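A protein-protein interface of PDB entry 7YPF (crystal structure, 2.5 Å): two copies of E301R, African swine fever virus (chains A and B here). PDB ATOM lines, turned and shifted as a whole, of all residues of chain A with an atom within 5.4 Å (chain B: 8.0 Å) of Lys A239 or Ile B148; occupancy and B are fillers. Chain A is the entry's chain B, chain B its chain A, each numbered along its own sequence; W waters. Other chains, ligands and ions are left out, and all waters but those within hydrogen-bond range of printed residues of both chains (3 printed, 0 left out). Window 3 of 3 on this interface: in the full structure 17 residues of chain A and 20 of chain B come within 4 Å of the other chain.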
ATOM      1  N   PHE A 188      -0.255 -28.474  -1.266  1.00  0.00           N
ATOM      2  CA  PHE A 188      -1.417 -29.263  -0.897  1.00  0.00           C
ATOM      3  C   PHE A 188      -1.218 -29.805   0.508  1.00  0.00           C
ATOM      4  O   PHE A 188      -0.091 -30.092   0.923  1.00  0.00           O
ATOM      5  CB  PHE A 188      -1.639 -30.448  -1.852  1.00  0.00           C
ATOM      6  CG  PHE A 188      -2.481 -30.126  -3.050  1.00  0.00           C
ATOM      7  CD1 PHE A 188      -3.205 -28.948  -3.117  1.00  0.00           C
ATOM      8  CD2 PHE A 188      -2.559 -31.017  -4.111  1.00  0.00           C
ATOM      9  CE1 PHE A 188      -3.983 -28.658  -4.224  1.00  0.00           C
ATOM     10  CE2 PHE A 188      -3.335 -30.734  -5.216  1.00  0.00           C
ATOM     11  CZ  PHE A 188      -4.047 -29.553  -5.275  1.00  0.00           C
ATOM     12  N   GLN A 192      -5.495 -33.430   0.743  1.00  0.00           N
ATOM     13  CA  GLN A 192      -5.876 -32.830  -0.532  1.00  0.00           C
ATOM     14  C   GLN A 192      -5.152 -33.506  -1.689  1.00  0.00           C
ATOM     15  O   GLN A 192      -5.753 -33.766  -2.737  1.00  0.00           O
ATOM     16  CB  GLN A 192      -5.585 -31.330  -0.522  1.00  0.00           C
ATOM     17  CG  GLN A 192      -6.640 -30.493   0.177  1.00  0.00           C
ATOM     18  CD  GLN A 192      -6.097 -29.163   0.662  1.00  0.00           C
ATOM     19  OE1 GLN A 192      -4.919 -28.853   0.472  1.00  0.00           O
ATOM     20  NE2 GLN A 192      -6.953 -28.371   1.295  1.00  0.00           N
ATOM     21  N   TYR A 234      -8.877 -24.648  -9.450  1.00  0.00           N
ATOM     22  CA  TYR A 234      -8.535 -23.971  -8.202  1.00  0.00           C
ATOM     23  C   TYR A 234      -8.685 -22.470  -8.427  1.00  0.00           C
ATOM     24  O   TYR A 234      -7.787 -21.819  -8.968  1.00  0.00           O
ATOM     25  CB  TYR A 234      -7.132 -24.365  -7.753  1.00  0.00           C
ATOM     26  CG  TYR A 234      -7.054 -25.828  -7.382  1.00  0.00           C
ATOM     27  CD1 TYR A 234      -6.913 -26.806  -8.358  1.00  0.00           C
ATOM     28  CD2 TYR A 234      -7.164 -26.234  -6.059  1.00  0.00           C
ATOM     29  CE1 TYR A 234      -6.862 -28.144  -8.024  1.00  0.00           C
ATOM     30  CE2 TYR A 234      -7.112 -27.569  -5.716  1.00  0.00           C
ATOM     31  CZ  TYR A 234      -6.962 -28.520  -6.703  1.00  0.00           C
ATOM     32  OH  TYR A 234      -6.912 -29.851  -6.363  1.00  0.00           O
ATOM     33  N   LYS A 235      -9.830 -21.932  -8.004  1.00  0.00           N
ATOM     34  CA  LYS A 235     -10.231 -20.569  -8.333  1.00  0.00           C
ATOM     35  C   LYS A 235      -9.567 -19.511  -7.462  1.00  0.00           C
ATOM     36  O   LYS A 235      -9.742 -18.319  -7.733  1.00  0.00           O
ATOM     37  CB  LYS A 235     -11.749 -20.435  -8.211  1.00  0.00           C
ATOM     38  CG  LYS A 235     -12.530 -21.444  -9.029  1.00  0.00           C
ATOM     39  CD  LYS A 235     -13.833 -20.843  -9.524  1.00  0.00           C
ATOM     40  CE  LYS A 235     -14.980 -21.183  -8.591  1.00  0.00           C
ATOM     41  NZ  LYS A 235     -16.086 -20.190  -8.687  1.00  0.00           N
ATOM     42  N   SER A 236      -8.830 -19.905  -6.427  1.00  0.00           N
ATOM     43  CA  SER A 236      -8.140 -18.962  -5.549  1.00  0.00           C
ATOM     44  C   SER A 236      -6.714 -19.461  -5.346  1.00  0.00           C
ATOM     45  O   SER A 236      -6.468 -20.328  -4.501  1.00  0.00           O
ATOM     46  CB  SER A 236      -8.873 -18.801  -4.222  1.00  0.00           C
ATOM     47  OG  SER A 236     -10.220 -18.415  -4.436  1.00  0.00           O
ATOM     48  N   SER A 237      -5.781 -18.913  -6.129  1.00  0.00           N
ATOM     49  CA  SER A 237      -4.386 -19.333  -6.045  1.00  0.00           C
ATOM     50  C   SER A 237      -3.810 -19.118  -4.651  1.00  0.00           C
ATOM     51  O   SER A 237      -2.953 -19.891  -4.208  1.00  0.00           O
ATOM     52  CB  SER A 237      -3.552 -18.582  -7.084  1.00  0.00           C
ATOM     53  OG  SER A 237      -3.995 -18.875  -8.399  1.00  0.00           O
ATOM     54  N   ASN A 238      -4.257 -18.071  -3.953  1.00  0.00           N
ATOM     55  CA  ASN A 238      -3.730 -17.777  -2.624  1.00  0.00           C
ATOM     56  C   ASN A 238      -4.037 -18.887  -1.623  1.00  0.00           C
ATOM     57  O   ASN A 238      -3.268 -19.097  -0.678  1.00  0.00           O
ATOM     58  CB  ASN A 238      -4.295 -16.446  -2.127  1.00  0.00           C
ATOM     59  CG  ASN A 238      -5.813 -16.414  -2.145  1.00  0.00           C
ATOM     60  OD1 ASN A 238      -6.439 -16.628  -3.184  1.00  0.00           O
ATOM     61  ND2 ASN A 238      -6.413 -16.142  -0.991  1.00  0.00           N
ATOM     62  N   LYS A 239      -5.144 -19.605  -1.807  1.00  0.00           N
ATOM     63  CA  LYS A 239      -5.538 -20.627  -0.845  1.00  0.00           C
ATOM     64  C   LYS A 239      -4.784 -21.940  -1.007  1.00  0.00           C
ATOM     65  O   LYS A 239      -4.862 -22.789  -0.113  1.00  0.00           O
ATOM     66  CB  LYS A 239      -7.045 -20.870  -0.929  1.00  0.00           C
ATOM     67  CG  LYS A 239      -7.847 -19.724  -0.338  1.00  0.00           C
ATOM     68  CD  LYS A 239      -9.320 -20.043  -0.240  1.00  0.00           C
ATOM     69  CE  LYS A 239     -10.096 -18.822   0.223  1.00  0.00           C
ATOM     70  NZ  LYS A 239     -11.559 -18.961  -0.009  1.00  0.00           N
ATOM     71  N   ILE A 240      -4.065 -22.133  -2.110  1.00  0.00           N
ATOM     72  CA  ILE A 240      -3.171 -23.272  -2.256  1.00  0.00           C
ATOM     73  C   ILE A 240      -1.715 -22.820  -2.371  1.00  0.00           C
ATOM     74  O   ILE A 240      -0.850 -23.602  -2.759  1.00  0.00           O
ATOM     75  CB  ILE A 240      -3.578 -24.158  -3.450  1.00  0.00           C
ATOM     76  CG1 ILE A 240      -3.731 -23.315  -4.717  1.00  0.00           C
ATOM     77  CG2 ILE A 240      -4.861 -24.914  -3.135  1.00  0.00           C
ATOM     78  CD1 ILE A 240      -3.680 -24.127  -5.994  1.00  0.00           C
ATOM     79  N   ASN A 241      -1.444 -21.563  -2.018  1.00  0.00           N
ATOM     80  CA  ASN A 241      -0.105 -20.978  -2.077  1.00  0.00           C
ATOM     81  C   ASN A 241       0.544 -21.216  -3.439  1.00  0.00           C
ATOM     82  O   ASN A 241       1.688 -21.663  -3.545  1.00  0.00           O
ATOM     83  CB  ASN A 241       0.774 -21.514  -0.947  1.00  0.00           C
ATOM     84  CG  ASN A 241       0.374 -20.968   0.410  1.00  0.00           C
ATOM     85  OD1 ASN A 241      -0.147 -19.857   0.515  1.00  0.00           O
ATOM     86  ND2 ASN A 241       0.613 -21.748   1.457  1.00  0.00           N
ATOM     87  N   SER B   2     -14.150 -17.509   1.600  1.00  0.00           N
ATOM     88  CA  SER B   2     -15.382 -16.861   2.016  1.00  0.00           C
ATOM     89  C   SER B   2     -15.389 -16.487   3.486  1.00  0.00           C
ATOM     90  O   SER B   2     -14.592 -15.661   3.928  1.00  0.00           O
ATOM     91  N   MET B   3     -16.302 -17.091   4.241  1.00  0.00           N
ATOM     92  CA  MET B   3     -16.359 -16.903   5.687  1.00  0.00           C
ATOM     93  C   MET B   3     -15.923 -18.196   6.367  1.00  0.00           C
ATOM     94  O   MET B   3     -16.558 -19.236   6.193  1.00  0.00           O
ATOM     95  CB  MET B   3     -17.768 -16.501   6.126  1.00  0.00           C
ATOM     96  CG  MET B   3     -18.094 -15.038   5.875  1.00  0.00           C
ATOM     97  SD  MET B   3     -17.994 -13.938   7.483  1.00  0.00           S
ATOM     98  CE  MET B   3     -19.894 -13.861   7.916  1.00  0.00           C
ATOM     99  N   SER B   4     -14.759 -18.158   7.009  1.00  0.00           N
ATOM    100  CA  SER B   4     -14.174 -19.354   7.612  1.00  0.00           C
ATOM    101  C   SER B   4     -13.635 -19.168   9.023  1.00  0.00           C
ATOM    102  O   SER B   4     -13.378 -18.048   9.465  1.00  0.00           O
ATOM    103  CB  SER B   4     -13.072 -19.916   6.709  1.00  0.00           C
ATOM    104  OG  SER B   4     -12.171 -20.724   7.445  1.00  0.00           O
ATOM    105  N   SER B 123     -15.420 -33.032   2.405  1.00  0.00           N
ATOM    106  CA  SER B 123     -14.722 -31.879   1.843  1.00  0.00           C
ATOM    107  C   SER B 123     -15.558 -31.131   0.810  1.00  0.00           C
ATOM    108  O   SER B 123     -15.214 -29.996   0.463  1.00  0.00           O
ATOM    109  CB  SER B 123     -13.396 -32.316   1.215  1.00  0.00           C
ATOM    110  OG  SER B 123     -13.593 -32.876  -0.073  1.00  0.00           O
ATOM    111  N   THR B 144     -18.011 -28.730  -5.026  1.00  0.00           N
ATOM    112  CA  THR B 144     -17.279 -27.540  -4.611  1.00  0.00           C
ATOM    113  C   THR B 144     -16.664 -27.763  -3.237  1.00  0.00           C
ATOM    114  O   THR B 144     -17.373 -28.087  -2.278  1.00  0.00           O
ATOM    115  CB  THR B 144     -18.192 -26.313  -4.597  1.00  0.00           C
ATOM    116  OG1 THR B 144     -18.814 -26.164  -5.879  1.00  0.00           O
ATOM    117  CG2 THR B 144     -17.394 -25.057  -4.278  1.00  0.00           C
ATOM    118  N   ASP B 145     -15.346 -27.581  -3.147  1.00  0.00           N
ATOM    119  CA  ASP B 145     -14.615 -27.586  -1.885  1.00  0.00           C
ATOM    120  C   ASP B 145     -14.346 -26.129  -1.515  1.00  0.00           C
ATOM    121  O   ASP B 145     -13.495 -25.475  -2.125  1.00  0.00           O
ATOM    122  CB  ASP B 145     -13.317 -28.386  -2.022  1.00  0.00           C
ATOM    123  CG  ASP B 145     -12.486 -28.422  -0.740  1.00  0.00           C
ATOM    124  OD1 ASP B 145     -12.536 -27.475   0.073  1.00  0.00           O
ATOM    125  OD2 ASP B 145     -11.758 -29.419  -0.551  1.00  0.00           O
ATOM    126  N   PHE B 146     -15.063 -25.627  -0.509  1.00  0.00           N
ATOM    127  CA  PHE B 146     -14.973 -24.215  -0.158  1.00  0.00           C
ATOM    128  C   PHE B 146     -13.728 -23.874   0.651  1.00  0.00           C
ATOM    129  O   PHE B 146     -13.375 -22.693   0.738  1.00  0.00           O
ATOM    130  CB  PHE B 146     -16.226 -23.784   0.601  1.00  0.00           C
ATOM    131  CG  PHE B 146     -17.422 -23.592  -0.281  1.00  0.00           C
ATOM    132  CD1 PHE B 146     -17.602 -22.408  -0.977  1.00  0.00           C
ATOM    133  CD2 PHE B 146     -18.361 -24.601  -0.427  1.00  0.00           C
ATOM    134  CE1 PHE B 146     -18.700 -22.228  -1.798  1.00  0.00           C
ATOM    135  CE2 PHE B 146     -19.462 -24.427  -1.245  1.00  0.00           C
ATOM    136  CZ  PHE B 146     -19.631 -23.238  -1.931  1.00  0.00           C
ATOM    137  N   ASP B 147     -13.066 -24.867   1.250  1.00  0.00           N
ATOM    138  CA  ASP B 147     -11.828 -24.592   1.971  1.00  0.00           C
ATOM    139  C   ASP B 147     -10.773 -23.979   1.056  1.00  0.00           C
ATOM    140  O   ASP B 147     -10.024 -23.087   1.471  1.00  0.00           O
ATOM    141  CB  ASP B 147     -11.294 -25.871   2.619  1.00  0.00           C
ATOM    142  CG  ASP B 147     -12.195 -26.388   3.723  1.00  0.00           C
ATOM    143  OD1 ASP B 147     -12.934 -25.576   4.319  1.00  0.00           O
ATOM    144  OD2 ASP B 147     -12.160 -27.606   3.998  1.00  0.00           O
ATOM    145  N   ILE B 148     -10.695 -24.443  -0.192  1.00  0.00           N
ATOM    146  CA  ILE B 148      -9.660 -23.982  -1.110  1.00  0.00           C
ATOM    147  C   ILE B 148     -10.267 -23.517  -2.430  1.00  0.00           C
ATOM    148  O   ILE B 148      -9.554 -23.365  -3.428  1.00  0.00           O
ATOM    149  CB  ILE B 148      -8.612 -25.085  -1.347  1.00  0.00           C
ATOM    150  CG1 ILE B 148      -9.300 -26.424  -1.615  1.00  0.00           C
ATOM    151  CG2 ILE B 148      -7.681 -25.205  -0.147  1.00  0.00           C
ATOM    152  CD1 ILE B 148      -8.351 -27.526  -2.036  1.00  0.00           C
ATOM    153  N   ASP B 149     -11.573 -23.257  -2.433  1.00  0.00           N
ATOM    154  CA  ASP B 149     -12.339 -22.934  -3.641  1.00  0.00           C
ATOM    155  C   ASP B 149     -11.940 -23.829  -4.814  1.00  0.00           C
ATOM    156  O   ASP B 149     -11.564 -23.370  -5.893  1.00  0.00           O
ATOM    157  CB  ASP B 149     -12.197 -21.460  -4.018  1.00  0.00           C
ATOM    158  CG  ASP B 149     -12.534 -20.530  -2.875  1.00  0.00           C
ATOM    159  OD1 ASP B 149     -13.734 -20.386  -2.559  1.00  0.00           O
ATOM    160  OD2 ASP B 149     -11.606 -19.924  -2.307  1.00  0.00           O
ATOM    161  N   LYS B 150     -12.037 -25.133  -4.581  1.00  0.00           N
ATOM    162  CA  LYS B 150     -11.773 -26.133  -5.605  1.00  0.00           C
ATOM    163  C   LYS B 150     -13.100 -26.589  -6.195  1.00  0.00           C
ATOM    164  O   LYS B 150     -13.971 -27.077  -5.467  1.00  0.00           O
ATOM    165  CB  LYS B 150     -11.004 -27.319  -5.024  1.00  0.00           C
ATOM    166  CG  LYS B 150     -10.840 -28.479  -5.985  1.00  0.00           C
ATOM    167  CD  LYS B 150      -9.999 -29.580  -5.363  1.00  0.00           C
ATOM    168  CE  LYS B 150     -10.785 -30.357  -4.323  1.00  0.00           C
ATOM    169  NZ  LYS B 150     -10.209 -31.710  -4.087  1.00  0.00           N
ATOM    170  N   GLU B 151     -13.254 -26.425  -7.506  1.00  0.00           N
ATOM    171  CA  GLU B 151     -14.437 -26.877  -8.228  1.00  0.00           C
ATOM    172  C   GLU B 151     -14.079 -28.116  -9.036  1.00  0.00           C
ATOM    173  O   GLU B 151     -13.162 -28.079  -9.864  1.00  0.00           O
ATOM    174  CB  GLU B 151     -14.984 -25.778  -9.137  1.00  0.00           C
ATOM    175  CG  GLU B 151     -16.245 -25.119  -8.607  1.00  0.00           C
ATOM    176  CD  GLU B 151     -16.857 -24.146  -9.592  1.00  0.00           C
ATOM    177  OE1 GLU B 151     -16.810 -24.423 -10.808  1.00  0.00           O
ATOM    178  OE2 GLU B 151     -17.397 -23.110  -9.151  1.00  0.00           O
HETATM  179  O   HOH W   1     -11.507 -16.773  -1.819  1.00  0.00           O
HETATM  180  O   HOH W   2      -8.092 -22.383  -5.291  1.00  0.00           O
HETATM  181  O   HOH W   3      -7.326 -31.271  -3.898  1.00  0.00           O
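The side-chain hydroxyl (OG) of Ser A236 lies within hydrogen-bond range of the side-chain carboxylate (OD2) of Asp B149 (3.0 Å). The side-chain amino group (NZ) of Lys A235 is in salt-bridge range of the side-chain carboxylate (OE2) of Glu B151 (3.2 Å). N of Ser B2 sits close to NZ of Lys A239 (3.4 Å). O of Asp B149 is in hydrogen-bond range of N of Lys A235. The side-chain amino group (NZ) of Lys A239 is in salt-bridge range of the side-chain carboxylate (OD2) of Asp B149 (2.5 Å).
The side-chain carboxylate of Asp B145 sits at hydrogen-bond distance from the backbone NH of Asp B147, at 2.9 Å. The backbone carbonyl oxygen (O) of Lys B150 lies within hydrogen-bond range of the backbone NH (N) of Asp B145, at 2.7 Å.
Among the printed residues, merely in contact across the chains: Gln A192 with Ile B148, Tyr A234 with Ile B148, Tyr A234 with Asp B149, Tyr A234 with Lys B150, Lys A239 with Asp B147 and Lys A239 with Ile B148.
Of the printed residues of chain B, Gln A192 touches Ile B148. Printed residues of chain B within 4 Å of Tyr A234: Ile B148, Asp B149 and Lys B150. Printed residues of chain B within 4 Å of Lys A235: Asp B149 and Glu B151. No residue of chain B comes within 4 Å of Asn A238. Lys A239 touches four residues of chain B. Asn A241 touches none of the printed residues of chain B. Thr B144 touches none of the printed residues of chain A. Ile B148 touches just these residues of chain A: Gln A192, Tyr A234 and Lys A239. Printed residues of chain A within 4 Å of Glu B151: Lys A235 (3.1 Å). The nearest printed residue of chain B that does not touch Tyr A234 is Glu B151 (5.1 Å).
Printed residues of chain B that touch a printed residue of chain A: Ser B2, Asp B147, Ile B148, Asp B149, Lys B150 and Glu B151. Hydrophobic or aromatic side chains of chain B that line the printed part of chain A: Ile B148. Printed residues of chain A that touch a printed residue of chain B: Gln A192, Tyr A234, Lys A235, Ser A236 and Lys A239. Hydrophobic or aromatic side chains of chain A within 4 Å of the printed part of chain B: Tyr A234. Among the printed residues, 11 pairs touch across the chains. Among the printed residues, Asp or Glu carboxylates within 4 Å of a Lys or Arg side-chain nitrogen of the other chain: Lys A235 with Glu B151 (3.2 Å) and Lys A239 with Asp B149 (2.5 Å).
No position is printed for both chains. Of the 11 pairs that touch across the chains among the printed residues, none has its exchanged pair printed and touching as well.
Water W2 lies within hydrogen-bond range of O of Ile B148, O of Ser A236 and N of Lys A235. Water W1 lies within hydrogen-bond range of NZ of Lys A239, OD2 of Asp B149 and OG of Ser A236. Water W3 lies within hydrogen-bond range of the side-chain hydroxyl of Tyr A234 (2.9 Å), the side-chain amino group of Lys B150 (2.9 Å) and the backbone carbonyl oxygen of Gln A192 (3.2 Å).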
